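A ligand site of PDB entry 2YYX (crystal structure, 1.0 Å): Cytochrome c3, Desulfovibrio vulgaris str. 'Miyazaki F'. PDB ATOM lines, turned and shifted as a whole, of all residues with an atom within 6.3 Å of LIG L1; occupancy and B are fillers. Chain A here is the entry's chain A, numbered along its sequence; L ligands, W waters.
C18 of LIG L1 is covalently linked to SG of Cys 100 (1.9 Å). The side-chain sulfur (SG) of Cys 105 is bonded to a carbon (C25) of LIG L1 (1.9 Å). An iron atom (FE1) of LIG L1 is bound by a ring nitrogen (NE2) of His 106 (2.0 Å). A ring nitrogen (NE2) of His 70 is bound to an iron atom (FE1) of LIG L1, 2.0 Å away. An oxygen (O4) of LIG L1 sits at hydrogen-bond distance from the backbone NH (N) of Thr 14. The side-chain hydroxyl (OG1) of Thr 14 sits at hydrogen-bond distance from an oxygen (O4) of LIG L1. N of Lys 13 sits at hydrogen-bond distance from O3 of LIG L1, at 2.9 Å. N of Asp 12 lies within hydrogen-bond range of O3 of LIG L1, at 3.3 Å. FE1 of LG2 L2 is bound by NE2 of His 83 (2.0 Å). The side-chain sulfur (SG) of Cys 79 is covalently linked to a carbon (C18) of LG2 L2 (1.8 Å).
The backbone NH (N) of Cys 105 sits close to the side-chain hydroxyl (OG) of Ser 103 (3.3 Å). ND1 of His 70 sits at hydrogen-bond distance from O of Tyr 66. The side-chain hydroxyl (OG1) of Thr 14 sits at hydrogen-bond distance from the backbone NH (N) of Gln 16 (2.9 Å). The backbone carbonyl oxygen (O) of Val 18 sits at hydrogen-bond distance from the backbone NH (N) of Met 11, at 2.8 Å. A ring nitrogen (ND1) of His 83 is in hydrogen-bond range of the backbone carbonyl oxygen (O) of Leu 97 (2.8 Å). OG of Ser 103 is in hydrogen-bond range of O of Gly 99, at 2.8 Å. The backbone carbonyl oxygen (O) of Met 69 sits close to the backbone NH (N) of Cys 79 (3.3 Å). N of Val 80 sits at hydrogen-bond distance from O of Met 69.
The backbone carbonyl oxygen (O) of Met 11 lies close to an oxygen (O4) of LIG L1, at 3.4 Å. O of Gln 16 touches C33 of LIG L1, 3.5 Å away. Pro 17 touches LIG L1 (CA to O4, 3.6 Å). Val 18 touches LIG L1 (CG2 to C28, 3.7 Å). O of Met 55 touches O2 of LIG L1, at 3.9 Å. Lys 57 touches LIG L1 (NZ to C9, 3.7 Å). Tyr 66 touches LIG L1. CG of Met 69 touches C31 of LIG L1 (3.9 Å). CB of Cys 79 touches C26 of LIG L1, at 3.6 Å. Val 80 touches LIG L1 (CG2 to C21, 3.7 Å). ND1 of His 83 touches C26 of LIG L1 (3.4 Å). Leu 97 touches LIG L1. Thr 98 touches LIG L1 (CA to C24, 3.5 Å). Gly 99 touches LIG L1. Hydrophobic or aromatic side chains that line LIG L1: Met 11, Val 18, Tyr 66, Met 69, His 70, Val 80, His 83 and His 106. 21 residues have an atom within 4 Å of LIG L1: Met 11, Asp 12, Lys 13, Thr 14, Gln 16, Pro 17, Val 18, Met 55, Lys 57, Tyr 66, Met 69, His 70, Cys 79, Val 80, His 83, Leu 97, Thr 98, Gly 99, Cys 100, Cys 105 and His 106. The nearest printed residue that does not touch LIG L1 is Ser 103 (4.1 Å).
Water W1 lies within hydrogen-bond range of O1 of LIG L1 (2.6 Å) and N of Lys 15 (2.9 Å). Water W4 lies within hydrogen-bond range of an oxygen (O2) of LIG L1 (2.6 Å) and the backbone carbonyl oxygen (O) of Met 55 (2.7 Å). Water W3 lies within hydrogen-bond range of an oxygen (O1) of LIG L1 and the side-chain amino group (NZ) of Lys 57.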
ATOM      1  N   MET A  11       1.897  -3.024 -28.931  1.00  0.00           N
ATOM      2  CA  MET A  11       0.476  -3.060 -29.300  1.00  0.00           C
ATOM      3  C   MET A  11       0.045  -1.591 -29.319  1.00  0.00           C
ATOM      4  O   MET A  11       0.114  -0.935 -28.292  1.00  0.00           O
ATOM      5  CB  MET A  11      -0.280  -3.863 -28.261  1.00  0.00           C
ATOM      6  CG  MET A  11       0.243  -5.317 -28.148  1.00  0.00           C
ATOM      7  SD  MET A  11      -0.597  -6.327 -26.923  1.00  0.00           S
ATOM      8  CE  MET A  11      -2.171  -6.594 -27.797  1.00  0.00           C
ATOM      9  N   ASP A  12      -0.365  -1.111 -30.495  1.00  0.00           N
ATOM     10  CA  ASP A  12      -0.495   0.319 -30.652  1.00  0.00           C
ATOM     11  C   ASP A  12      -1.671   0.739 -31.528  1.00  0.00           C
ATOM     12  O   ASP A  12      -1.619   1.718 -32.272  1.00  0.00           O
ATOM     13  CB  ASP A  12       0.830   0.876 -31.263  1.00  0.00           C
ATOM     14  CG  ASP A  12       1.185   0.192 -32.574  1.00  0.00           C
ATOM     15  OD1 ASP A  12       0.348  -0.489 -33.172  1.00  0.00           O
ATOM     16  OD2 ASP A  12       2.368   0.401 -33.034  1.00  0.00           O
ATOM     17  N   LYS A  13      -2.773  -0.001 -31.374  1.00  0.00           N
ATOM     18  CA  LYS A  13      -3.993   0.461 -32.025  1.00  0.00           C
ATOM     19  C   LYS A  13      -4.679   1.630 -31.386  1.00  0.00           C
ATOM     20  O   LYS A  13      -5.588   2.268 -32.004  1.00  0.00           O
ATOM     21  CB  LYS A  13      -5.030  -0.700 -32.066  1.00  0.00           C
ATOM     22  CG  LYS A  13      -4.550  -1.915 -32.872  1.00  0.00           C
ATOM     23  CD  LYS A  13      -4.501  -1.533 -34.354  1.00  0.00           C
ATOM     24  CE  LYS A  13      -4.299  -2.590 -35.400  1.00  0.00           C
ATOM     25  NZ  LYS A  13      -5.007  -2.162 -36.646  1.00  0.00           N
ATOM     26  N   THR A  14      -4.334   1.968 -30.154  1.00  0.00           N
ATOM     27  CA  THR A  14      -4.987   2.963 -29.375  1.00  0.00           C
ATOM     28  C   THR A  14      -4.033   4.072 -28.906  1.00  0.00           C
ATOM     29  O   THR A  14      -2.806   3.942 -29.127  1.00  0.00           O
ATOM     30  CB  THR A  14      -5.670   2.362 -28.122  1.00  0.00           C
ATOM     31  OG1 THR A  14      -4.689   2.163 -27.087  1.00  0.00           O
ATOM     32  CG2 THR A  14      -6.379   1.039 -28.449  1.00  0.00           C
ATOM     33  N   LYS A  15      -4.553   5.074 -28.225  1.00  0.00           N
ATOM     34  CA  LYS A  15      -3.699   6.096 -27.624  1.00  0.00           C
ATOM     35  C   LYS A  15      -3.081   5.669 -26.294  1.00  0.00           C
ATOM     36  O   LYS A  15      -2.375   6.465 -25.680  1.00  0.00           O
ATOM     37  CB  LYS A  15      -4.444   7.412 -27.479  1.00  0.00           C
ATOM     38  CG  LYS A  15      -4.880   7.976 -28.873  1.00  0.00           C
ATOM     39  CD  LYS A  15      -5.462   9.341 -28.702  1.00  0.00           C
ATOM     40  CE  LYS A  15      -6.034   9.812 -30.035  1.00  0.00           C
ATOM     41  NZ  LYS A  15      -6.625  11.176 -29.866  1.00  0.00           N
ATOM     42  N   GLN A  16      -3.299   4.411 -25.913  1.00  0.00           N
ATOM     43  CA  GLN A  16      -2.703   3.869 -24.702  1.00  0.00           C
ATOM     44  C   GLN A  16      -1.929   2.599 -25.060  1.00  0.00           C
ATOM     45  O   GLN A  16      -2.244   1.515 -24.619  1.00  0.00           O
ATOM     46  CB  GLN A  16      -3.848   3.565 -23.684  1.00  0.00           C
ATOM     47  CG  GLN A  16      -4.861   4.665 -23.505  1.00  0.00           C
ATOM     48  CD  GLN A  16      -4.339   6.026 -23.097  1.00  0.00           C
ATOM     49  OE1 GLN A  16      -3.287   6.097 -22.465  1.00  0.00           O
ATOM     50  NE2 GLN A  16      -5.076   7.055 -23.398  1.00  0.00           N
ATOM     51  N   PRO A  17      -0.862   2.782 -25.832  1.00  0.00           N
ATOM     52  CA  PRO A  17      -0.126   1.576 -26.339  1.00  0.00           C
ATOM     53  C   PRO A  17       0.571   0.807 -25.225  1.00  0.00           C
ATOM     54  O   PRO A  17       0.984   1.346 -24.192  1.00  0.00           O
ATOM     55  CB  PRO A  17       0.903   2.192 -27.292  1.00  0.00           C
ATOM     56  CG  PRO A  17       1.101   3.579 -26.780  1.00  0.00           C
ATOM     57  CD  PRO A  17      -0.279   4.020 -26.364  1.00  0.00           C
ATOM     58  N   VAL A  18       0.720  -0.531 -25.459  1.00  0.00           N
ATOM     59  CA  VAL A  18       1.276  -1.431 -24.425  1.00  0.00           C
ATOM     60  C   VAL A  18       2.325  -2.311 -25.055  1.00  0.00           C
ATOM     61  O   VAL A  18       2.155  -2.785 -26.155  1.00  0.00           O
ATOM     62  CB  VAL A  18       0.124  -2.292 -23.867  1.00  0.00           C
ATOM     63  CG1 VAL A  18       0.611  -3.353 -22.895  1.00  0.00           C
ATOM     64  CG2 VAL A  18      -0.898  -1.401 -23.180  1.00  0.00           C
ATOM     65  N   MET A  55     -13.257  -0.790 -32.226  1.00  0.00           N
ATOM     66  CA  MET A  55     -12.439   0.098 -31.418  1.00  0.00           C
ATOM     67  C   MET A  55     -13.240   0.978 -30.456  1.00  0.00           C
ATOM     68  O   MET A  55     -12.686   1.926 -29.896  1.00  0.00           O
ATOM     69  CB  MET A  55     -11.464   0.870 -32.306  1.00  0.00           C
ATOM     70  CG  MET A  55     -10.696  -0.159 -33.174  1.00  0.00           C
ATOM     71  SD  MET A  55      -9.902  -1.656 -32.417  1.00  0.00           S
ATOM     72  CE  MET A  55      -8.951  -0.630 -31.253  1.00  0.00           C
ATOM     73  N   ASP A  56     -14.528   0.645 -30.253  1.00  0.00           N
ATOM     74  CA  ASP A  56     -15.320   1.246 -29.209  1.00  0.00           C
ATOM     75  C   ASP A  56     -15.076   0.466 -27.892  1.00  0.00           C
ATOM     76  O   ASP A  56     -15.451  -0.715 -27.791  1.00  0.00           O
ATOM     77  CB  ASP A  56     -16.785   1.278 -29.557  1.00  0.00           C
ATOM     78  CG  ASP A  56     -17.567   2.033 -28.464  1.00  0.00           C
ATOM     79  OD1 ASP A  56     -17.736   1.547 -27.367  1.00  0.00           O
ATOM     80  OD2 ASP A  56     -17.998   3.201 -28.688  1.00  0.00           O
ATOM     81  N   LYS A  57     -14.509   1.148 -26.899  1.00  0.00           N
ATOM     82  CA  LYS A  57     -14.041   0.443 -25.711  1.00  0.00           C
ATOM     83  C   LYS A  57     -15.168   0.019 -24.801  1.00  0.00           C
ATOM     84  O   LYS A  57     -14.873  -0.643 -23.801  1.00  0.00           O
ATOM     85  CB  LYS A  57     -12.964   1.296 -24.989  1.00  0.00           C
ATOM     86  CG  LYS A  57     -13.513   2.558 -24.378  1.00  0.00           C
ATOM     87  CD  LYS A  57     -12.379   3.311 -23.620  1.00  0.00           C
ATOM     88  CE  LYS A  57     -12.837   4.707 -23.222  1.00  0.00           C
ATOM     89  NZ  LYS A  57     -11.719   5.447 -22.529  1.00  0.00           N
ATOM     90  N   TYR A  66     -11.129  -3.654 -26.674  1.00  0.00           N
ATOM     91  CA  TYR A  66     -10.940  -3.369 -25.259  1.00  0.00           C
ATOM     92  C   TYR A  66     -11.381  -4.568 -24.445  1.00  0.00           C
ATOM     93  O   TYR A  66     -10.730  -5.016 -23.499  1.00  0.00           O
ATOM     94  CB  TYR A  66     -11.659  -2.070 -24.886  1.00  0.00           C
ATOM     95  CG  TYR A  66     -11.487  -1.736 -23.415  1.00  0.00           C
ATOM     96  CD1 TYR A  66     -12.297  -2.301 -22.412  1.00  0.00           C
ATOM     97  CD2 TYR A  66     -10.460  -0.837 -23.023  1.00  0.00           C
ATOM     98  CE1 TYR A  66     -12.123  -1.993 -21.084  1.00  0.00           C
ATOM     99  CE2 TYR A  66     -10.297  -0.547 -21.681  1.00  0.00           C
ATOM    100  CZ  TYR A  66     -11.106  -1.125 -20.717  1.00  0.00           C
ATOM    101  OH  TYR A  66     -10.922  -0.791 -19.406  1.00  0.00           O
ATOM    102  N   MET A  69      -9.104  -7.567 -24.138  1.00  0.00           N
ATOM    103  CA  MET A  69      -7.864  -7.436 -23.359  1.00  0.00           C
ATOM    104  C   MET A  69      -8.107  -7.167 -21.886  1.00  0.00           C
ATOM    105  O   MET A  69      -7.213  -7.411 -21.096  1.00  0.00           O
ATOM    106  CB  MET A  69      -7.013  -6.278 -23.894  1.00  0.00           C
ATOM    107  CG  MET A  69      -6.676  -5.948 -25.297  1.00  0.00           C
ATOM    108  SD  MET A  69      -5.674  -7.062 -26.048  1.00  0.00           S
ATOM    109  CE  MET A  69      -5.792  -6.914 -27.821  1.00  0.00           C
ATOM    110  N   HIS A  70      -9.318  -6.708 -21.508  1.00  0.00           N
ATOM    111  CA  HIS A  70      -9.522  -6.205 -20.165  1.00  0.00           C
ATOM    112  C   HIS A  70     -10.558  -6.985 -19.323  1.00  0.00           C
ATOM    113  O   HIS A  70     -10.508  -6.834 -18.095  1.00  0.00           O
ATOM    114  CB  HIS A  70      -9.940  -4.734 -20.149  1.00  0.00           C
ATOM    115  CG  HIS A  70      -8.902  -3.795 -20.707  1.00  0.00           C
ATOM    116  ND1 HIS A  70      -8.772  -3.593 -22.078  1.00  0.00           N
ATOM    117  CD2 HIS A  70      -7.958  -3.030 -20.131  1.00  0.00           C
ATOM    118  CE1 HIS A  70      -7.777  -2.720 -22.291  1.00  0.00           C
ATOM    119  NE2 HIS A  70      -7.262  -2.355 -21.101  1.00  0.00           N
ATOM    120  N   CYS A  79      -5.886 -10.456 -21.046  1.00  0.00           N
ATOM    121  CA  CYS A  79      -4.691  -9.986 -20.355  1.00  0.00           C
ATOM    122  C   CYS A  79      -4.983  -9.701 -18.857  1.00  0.00           C
ATOM    123  O   CYS A  79      -4.313 -10.227 -17.957  1.00  0.00           O
ATOM    124  CB  CYS A  79      -4.173  -8.660 -20.931  1.00  0.00           C
ATOM    125  SG  CYS A  79      -4.039  -8.497 -22.732  1.00  0.00           S
ATOM    126  N   VAL A  80      -6.002  -8.871 -18.635  1.00  0.00           N
ATOM    127  CA  VAL A  80      -6.315  -8.494 -17.237  1.00  0.00           C
ATOM    128  C   VAL A  80      -6.871  -9.692 -16.463  1.00  0.00           C
ATOM    129  O   VAL A  80      -6.510  -9.869 -15.289  1.00  0.00           O
ATOM    130  CB  VAL A  80      -7.268  -7.310 -17.199  1.00  0.00           C
ATOM    131  CG1 VAL A  80      -7.725  -7.001 -15.761  1.00  0.00           C
ATOM    132  CG2 VAL A  80      -6.608  -6.049 -17.772  1.00  0.00           C
ATOM    133  N   HIS A  83      -4.095 -11.914 -15.437  1.00  0.00           N
ATOM    134  CA  HIS A  83      -3.280 -11.255 -14.427  1.00  0.00           C
ATOM    135  C   HIS A  83      -3.969 -11.177 -13.071  1.00  0.00           C
ATOM    136  O   HIS A  83      -3.305 -11.243 -12.028  1.00  0.00           O
ATOM    137  CB  HIS A  83      -2.930  -9.822 -14.907  1.00  0.00           C
ATOM    138  CG  HIS A  83      -1.872  -9.851 -15.991  1.00  0.00           C
ATOM    139  ND1 HIS A  83      -1.264  -8.652 -16.331  1.00  0.00           N
ATOM    140  CD2 HIS A  83      -1.330 -10.771 -16.780  1.00  0.00           C
ATOM    141  CE1 HIS A  83      -0.424  -8.895 -17.326  1.00  0.00           C
ATOM    142  NE2 HIS A  83      -0.403 -10.196 -17.616  1.00  0.00           N
ATOM    143  N   LYS A  95      -1.670  -4.155  -8.371  1.00  0.00           N
ATOM    144  CA  LYS A  95      -1.391  -2.850  -8.968  1.00  0.00           C
ATOM    145  C   LYS A  95      -0.474  -3.006 -10.188  1.00  0.00           C
ATOM    146  O   LYS A  95      -0.719  -2.412 -11.240  1.00  0.00           O
ATOM    147  CB  LYS A  95      -0.754  -1.957  -7.895  1.00  0.00           C
ATOM    148  CG  LYS A  95      -0.134  -0.681  -8.386  1.00  0.00           C
ATOM    149  CD  LYS A  95      -1.157   0.298  -8.915  1.00  0.00           C
ATOM    150  CE  LYS A  95      -0.475   1.650  -9.156  1.00  0.00           C
ATOM    151  NZ  LYS A  95      -1.403   2.634  -9.749  1.00  0.00           N
ATOM    152  N   GLU A  96       0.608  -3.802 -10.004  1.00  0.00           N
ATOM    153  CA  GLU A  96       1.547  -3.993 -11.110  1.00  0.00           C
ATOM    154  C   GLU A  96       0.975  -4.614 -12.362  1.00  0.00           C
ATOM    155  O   GLU A  96       1.280  -4.248 -13.494  1.00  0.00           O
ATOM    156  CB  GLU A  96       2.657  -4.868 -10.570  1.00  0.00           C
ATOM    157  CG  GLU A  96       3.397  -5.922 -11.287  1.00  0.00           C
ATOM    158  CD  GLU A  96       4.522  -6.534 -10.439  1.00  0.00           C
ATOM    159  OE1 GLU A  96       5.163  -7.468 -10.906  1.00  0.00           O
ATOM    160  OE2 GLU A  96       4.749  -6.078  -9.307  1.00  0.00           O
ATOM    161  N   LEU A  97       0.101  -5.619 -12.153  1.00  0.00           N
ATOM    162  CA  LEU A  97      -0.340  -6.433 -13.277  1.00  0.00           C
ATOM    163  C   LEU A  97      -1.756  -6.074 -13.761  1.00  0.00           C
ATOM    164  O   LEU A  97      -2.091  -6.464 -14.866  1.00  0.00           O
ATOM    165  CB  LEU A  97      -0.295  -7.906 -12.890  1.00  0.00           C
ATOM    166  CG  LEU A  97       1.057  -8.481 -12.504  1.00  0.00           C
ATOM    167  CD1 LEU A  97       0.917  -9.942 -12.081  1.00  0.00           C
ATOM    168  CD2 LEU A  97       2.038  -8.333 -13.676  1.00  0.00           C
ATOM    169  N   THR A  98      -2.519  -5.354 -12.932  1.00  0.00           N
ATOM    170  CA  THR A  98      -3.914  -5.055 -13.284  1.00  0.00           C
ATOM    171  C   THR A  98      -4.276  -3.591 -13.143  1.00  0.00           C
ATOM    172  O   THR A  98      -5.407  -3.218 -13.570  1.00  0.00           O
ATOM    173  CB  THR A  98      -4.999  -5.909 -12.560  1.00  0.00           C
ATOM    174  OG1 THR A  98      -5.131  -5.522 -11.194  1.00  0.00           O
ATOM    175  CG2 THR A  98      -4.646  -7.405 -12.735  1.00  0.00           C
ATOM    176  N   GLY A  99      -3.379  -2.738 -12.640  1.00  0.00           N
ATOM    177  CA  GLY A  99      -3.716  -1.344 -12.427  1.00  0.00           C
ATOM    178  C   GLY A  99      -3.949  -0.639 -13.749  1.00  0.00           C
ATOM    179  O   GLY A  99      -3.311  -0.889 -14.761  1.00  0.00           O
ATOM    180  N   CYS A 100      -4.892   0.304 -13.707  1.00  0.00           N
ATOM    181  CA  CYS A 100      -5.208   1.024 -14.937  1.00  0.00           C
ATOM    182  C   CYS A 100      -4.174   2.102 -15.270  1.00  0.00           C
ATOM    183  O   CYS A 100      -4.077   2.493 -16.451  1.00  0.00           O
ATOM    184  CB  CYS A 100      -6.592   1.695 -14.843  1.00  0.00           C
ATOM    185  SG  CYS A 100      -7.891   0.541 -14.379  1.00  0.00           S
ATOM    186  N   LYS A 101      -3.470   2.585 -14.264  1.00  0.00           N
ATOM    187  CA  LYS A 101      -2.355   3.499 -14.438  1.00  0.00           C
ATOM    188  C   LYS A 101      -1.248   3.051 -13.507  1.00  0.00           C
ATOM    189  O   LYS A 101      -1.539   2.347 -12.533  1.00  0.00           O
ATOM    190  CB  LYS A 101      -2.731   4.946 -14.123  1.00  0.00           C
ATOM    191  CG  LYS A 101      -3.273   5.081 -12.715  1.00  0.00           C
ATOM    192  CD  LYS A 101      -4.098   6.368 -12.613  1.00  0.00           C
ATOM    193  CE  LYS A 101      -4.095   6.897 -11.194  1.00  0.00           C
ATOM    194  NZ  LYS A 101      -2.662   7.100 -10.832  1.00  0.00           N
ATOM    195  N   SER A 103       0.883   0.834 -13.865  1.00  0.00           N
ATOM    196  CA  SER A 103       1.078  -0.599 -13.918  1.00  0.00           C
ATOM    197  C   SER A 103       2.100  -0.951 -14.983  1.00  0.00           C
ATOM    198  O   SER A 103       2.639  -0.105 -15.702  1.00  0.00           O
ATOM    199  CB  SER A 103      -0.249  -1.298 -14.234  1.00  0.00           C
ATOM    200  OG  SER A 103      -0.684  -1.001 -15.573  1.00  0.00           O
ATOM    201  N   LYS A 104       2.356  -2.274 -15.098  1.00  0.00           N
ATOM    202  CA  LYS A 104       3.290  -2.723 -16.123  1.00  0.00           C
ATOM    203  C   LYS A 104       2.706  -2.596 -17.532  1.00  0.00           C
ATOM    204  O   LYS A 104       3.451  -2.599 -18.520  1.00  0.00           O
ATOM    205  CB  LYS A 104       3.774  -4.145 -15.846  1.00  0.00           C
ATOM    206  CG  LYS A 104       4.646  -4.110 -14.535  1.00  0.00           C
ATOM    207  CD  LYS A 104       5.113  -5.430 -14.047  1.00  0.00           C
ATOM    208  CE  LYS A 104       6.195  -5.188 -12.976  1.00  0.00           C
ATOM    209  NZ  LYS A 104       7.556  -5.439 -13.513  1.00  0.00           N
ATOM    210  N   CYS A 105       1.385  -2.467 -17.648  1.00  0.00           N
ATOM    211  CA  CYS A 105       0.771  -2.247 -18.965  1.00  0.00           C
ATOM    212  C   CYS A 105       0.645  -0.783 -19.305  1.00  0.00           C
ATOM    213  O   CYS A 105       1.027  -0.379 -20.429  1.00  0.00           O
ATOM    214  CB  CYS A 105      -0.642  -2.879 -19.065  1.00  0.00           C
ATOM    215  SG  CYS A 105      -0.538  -4.654 -18.771  1.00  0.00           S
ATOM    216  N   HIS A 106       0.151   0.042 -18.398  1.00  0.00           N
ATOM    217  CA  HIS A 106      -0.087   1.473 -18.626  1.00  0.00           C
ATOM    218  C   HIS A 106       0.660   2.332 -17.611  1.00  0.00           C
ATOM    219  O   HIS A 106       0.401   2.239 -16.426  1.00  0.00           O
ATOM    220  CB  HIS A 106      -1.565   1.807 -18.513  1.00  0.00           C
ATOM    221  CG  HIS A 106      -2.464   1.098 -19.528  1.00  0.00           C
ATOM    222  ND1 HIS A 106      -2.324   1.209 -20.889  1.00  0.00           N
ATOM    223  CD2 HIS A 106      -3.574   0.341 -19.328  1.00  0.00           C
ATOM    224  CE1 HIS A 106      -3.339   0.505 -21.460  1.00  0.00           C
ATOM    225  NE2 HIS A 106      -4.124  -0.026 -20.548  1.00  0.00           N
HETATM  226  C1  LIG L   1      -5.802  -0.186 -24.107  1.00  0.00           C
HETATM  227  C2  LIG L   1      -7.821   1.424 -20.068  1.00  0.00           C
HETATM  228  C3  LIG L   1      -5.557  -1.955 -17.525  1.00  0.00           C
HETATM  229  C4  LIG L   1      -3.721  -3.723 -21.624  1.00  0.00           C
HETATM  230  C5  LIG L   1      -6.495   0.614 -23.211  1.00  0.00           C
HETATM  231  C6  LIG L   1      -7.195   1.795 -23.540  1.00  0.00           C
HETATM  232  C7  LIG L   1      -7.718   2.271 -22.378  1.00  0.00           C
HETATM  233  C8  LIG L   1      -7.331   1.363 -21.372  1.00  0.00           C
HETATM  234  C9  LIG L   1      -8.584   3.512 -22.153  1.00  0.00           C
HETATM  235  C10 LIG L   1      -7.398   2.414 -24.903  1.00  0.00           C
HETATM  236  C11 LIG L   1      -8.788   1.976 -25.470  1.00  0.00           C
HETATM  237  C12 LIG L   1      -9.142   2.765 -26.709  1.00  0.00           C
HETATM  238  O1  LIG L   1      -9.112   4.034 -26.645  1.00  0.00           O
HETATM  239  O2  LIG L   1      -9.489   2.180 -27.733  1.00  0.00           O
HETATM  240  C13 LIG L   1      -7.493   0.525 -19.027  1.00  0.00           C
HETATM  241  C14 LIG L   1      -8.078   0.571 -17.753  1.00  0.00           C
HETATM  242  C15 LIG L   1      -7.415  -0.384 -16.997  1.00  0.00           C
HETATM  243  C16 LIG L   1      -6.485  -0.973 -17.870  1.00  0.00           C
HETATM  244  C17 LIG L   1      -9.180   1.554 -17.375  1.00  0.00           C
HETATM  245  C18 LIG L   1      -7.672  -0.822 -15.614  1.00  0.00           C
HETATM  246  C19 LIG L   1      -8.886  -1.711 -15.474  1.00  0.00           C
HETATM  247  C20 LIG L   1      -4.737  -2.685 -18.423  1.00  0.00           C
HETATM  248  C21 LIG L   1      -3.783  -3.620 -18.033  1.00  0.00           C
HETATM  249  C22 LIG L   1      -3.256  -4.172 -19.170  1.00  0.00           C
HETATM  250  C23 LIG L   1      -3.917  -3.478 -20.262  1.00  0.00           C
HETATM  251  C24 LIG L   1      -3.414  -3.914 -16.581  1.00  0.00           C
HETATM  252  C25 LIG L   1      -2.237  -5.183 -19.333  1.00  0.00           C
HETATM  253  C26 LIG L   1      -2.499  -6.507 -18.607  1.00  0.00           C
HETATM  254  C27 LIG L   1      -4.192  -2.982 -22.673  1.00  0.00           C
HETATM  255  C28 LIG L   1      -3.929  -3.257 -24.041  1.00  0.00           C
HETATM  256  C29 LIG L   1      -4.517  -2.222 -24.760  1.00  0.00           C
HETATM  257  C30 LIG L   1      -5.107  -1.387 -23.838  1.00  0.00           C
HETATM  258  C31 LIG L   1      -3.121  -4.451 -24.556  1.00  0.00           C
HETATM  259  C32 LIG L   1      -4.401  -1.994 -26.273  1.00  0.00           C
HETATM  260  C33 LIG L   1      -3.135  -1.229 -26.631  1.00  0.00           C
HETATM  261  C34 LIG L   1      -3.095  -0.762 -28.078  1.00  0.00           C
HETATM  262  O3  LIG L   1      -3.325  -1.557 -28.993  1.00  0.00           O
HETATM  263  O4  LIG L   1      -2.955   0.485 -28.227  1.00  0.00           O
HETATM  264  N1  LIG L   1      -6.598   0.355 -21.890  1.00  0.00           N
HETATM  265  N2  LIG L   1      -6.588  -0.455 -19.110  1.00  0.00           N
HETATM  266  N3  LIG L   1      -4.763  -2.573 -19.783  1.00  0.00           N
HETATM  267  N4  LIG L   1      -4.936  -1.848 -22.566  1.00  0.00           N
HETATM  268 FE1  LIG L   1      -5.712  -1.134 -20.842  1.00  0.00          FE
HETATM  269  C1  LG2 L   2       3.379 -10.518 -16.891  1.00  0.00           C
HETATM  270  C2  LG2 L   2       1.238  -7.902 -20.282  1.00  0.00           C
HETATM  271  C3  LG2 L   2      -1.739 -11.604 -21.207  1.00  0.00           C
HETATM  272  C4  LG2 L   2       0.200 -14.088 -17.574  1.00  0.00           C
HETATM  273  C5  LG2 L   2       3.080  -9.467 -17.769  1.00  0.00           C
HETATM  274  C6  LG2 L   2       3.751  -8.232 -17.791  1.00  0.00           C
HETATM  275  C7  LG2 L   2       3.112  -7.476 -18.735  1.00  0.00           C
HETATM  276  C8  LG2 L   2       2.121  -8.311 -19.290  1.00  0.00           C
HETATM  277  C9  LG2 L   2       3.379  -6.050 -19.158  1.00  0.00           C
HETATM  278  C10 LG2 L   2       4.948  -7.822 -16.929  1.00  0.00           C
HETATM  279  C11 LG2 L   2       6.256  -8.439 -17.480  1.00  0.00           C
HETATM  280  C12 LG2 L   2       6.576  -7.850 -18.863  1.00  0.00           C
HETATM  281  O1  LG2 L   2       6.820  -6.634 -18.901  1.00  0.00           O
HETATM  282  O2  LG2 L   2       6.549  -8.592 -19.842  1.00  0.00           O
HETATM  283  C13 LG2 L   2       0.225  -8.701 -20.854  1.00  0.00           C
HETATM  284  C14 LG2 L   2      -0.657  -8.289 -21.901  1.00  0.00           C
HETATM  285  C15 LG2 L   2      -1.454  -9.349 -22.215  1.00  0.00           C
HETATM  286  C16 LG2 L   2      -1.084 -10.358 -21.258  1.00  0.00           C
HETATM  287  C17 LG2 L   2      -0.623  -6.885 -22.570  1.00  0.00           C
HETATM  288  C18 LG2 L   2      -2.539  -9.475 -23.194  1.00  0.00           C
HETATM  289  C19 LG2 L   2      -2.171  -9.042 -24.612  1.00  0.00           C
HETATM  290  C20 LG2 L   2      -1.499 -12.594 -20.234  1.00  0.00           C
HETATM  291  C21 LG2 L   2      -2.305 -13.766 -20.094  1.00  0.00           C
HETATM  292  C22 LG2 L   2      -1.785 -14.485 -19.051  1.00  0.00           C
HETATM  293  C23 LG2 L   2      -0.673 -13.677 -18.564  1.00  0.00           C
HETATM  294  C24 LG2 L   2      -3.492 -14.036 -21.041  1.00  0.00           C
HETATM  295  C25 LG2 L   2      -2.168 -15.749 -18.471  1.00  0.00           C
HETATM  296  C26 LG2 L   2      -2.986 -16.743 -19.310  1.00  0.00           C
HETATM  297  C27 LG2 L   2       1.303 -13.339 -17.104  1.00  0.00           C
HETATM  298  C28 LG2 L   2       2.144 -13.762 -16.053  1.00  0.00           C
HETATM  299  C29 LG2 L   2       3.081 -12.753 -15.882  1.00  0.00           C
HETATM  300  C30 LG2 L   2       2.721 -11.754 -16.779  1.00  0.00           C
HETATM  301  C31 LG2 L   2       2.013 -15.085 -15.316  1.00  0.00           C
HETATM  302  C32 LG2 L   2       4.196 -12.686 -14.865  1.00  0.00           C
HETATM  303  C33 LG2 L   2       3.667 -11.990 -13.613  1.00  0.00           C
HETATM  304  C34 LG2 L   2       4.746 -11.393 -12.743  1.00  0.00           C
HETATM  305  O3  LG2 L   2       4.549 -11.233 -11.570  1.00  0.00           O
HETATM  306  O4  LG2 L   2       5.750 -10.844 -13.292  1.00  0.00           O
HETATM  307  N1  LG2 L   2       2.073  -9.504 -18.682  1.00  0.00           N
HETATM  308  N2  LG2 L   2      -0.056  -9.960 -20.467  1.00  0.00           N
HETATM  309  N3  LG2 L   2      -0.564 -12.538 -19.281  1.00  0.00           N
HETATM  310  N4  LG2 L   2       1.658 -12.118 -17.525  1.00  0.00           N
HETATM  311 FE1  LG2 L   2       0.777 -11.031 -18.983  1.00  0.00          FE
HETATM  312  O   HOH W   1      -7.339   5.555 -27.863  1.00  0.00           O
HETATM  313  O   HOH W   2     -11.404   4.022 -20.188  1.00  0.00           O
HETATM  314  O   HOH W   3      -9.896   5.728 -24.741  1.00  0.00           O
HETATM  315  O   HOH W   4     -10.157   2.963 -30.163  1.00  0.00           O
HETATM  316  O   HOH W   5      -9.968  -0.447 -28.112  1.00  0.00           O
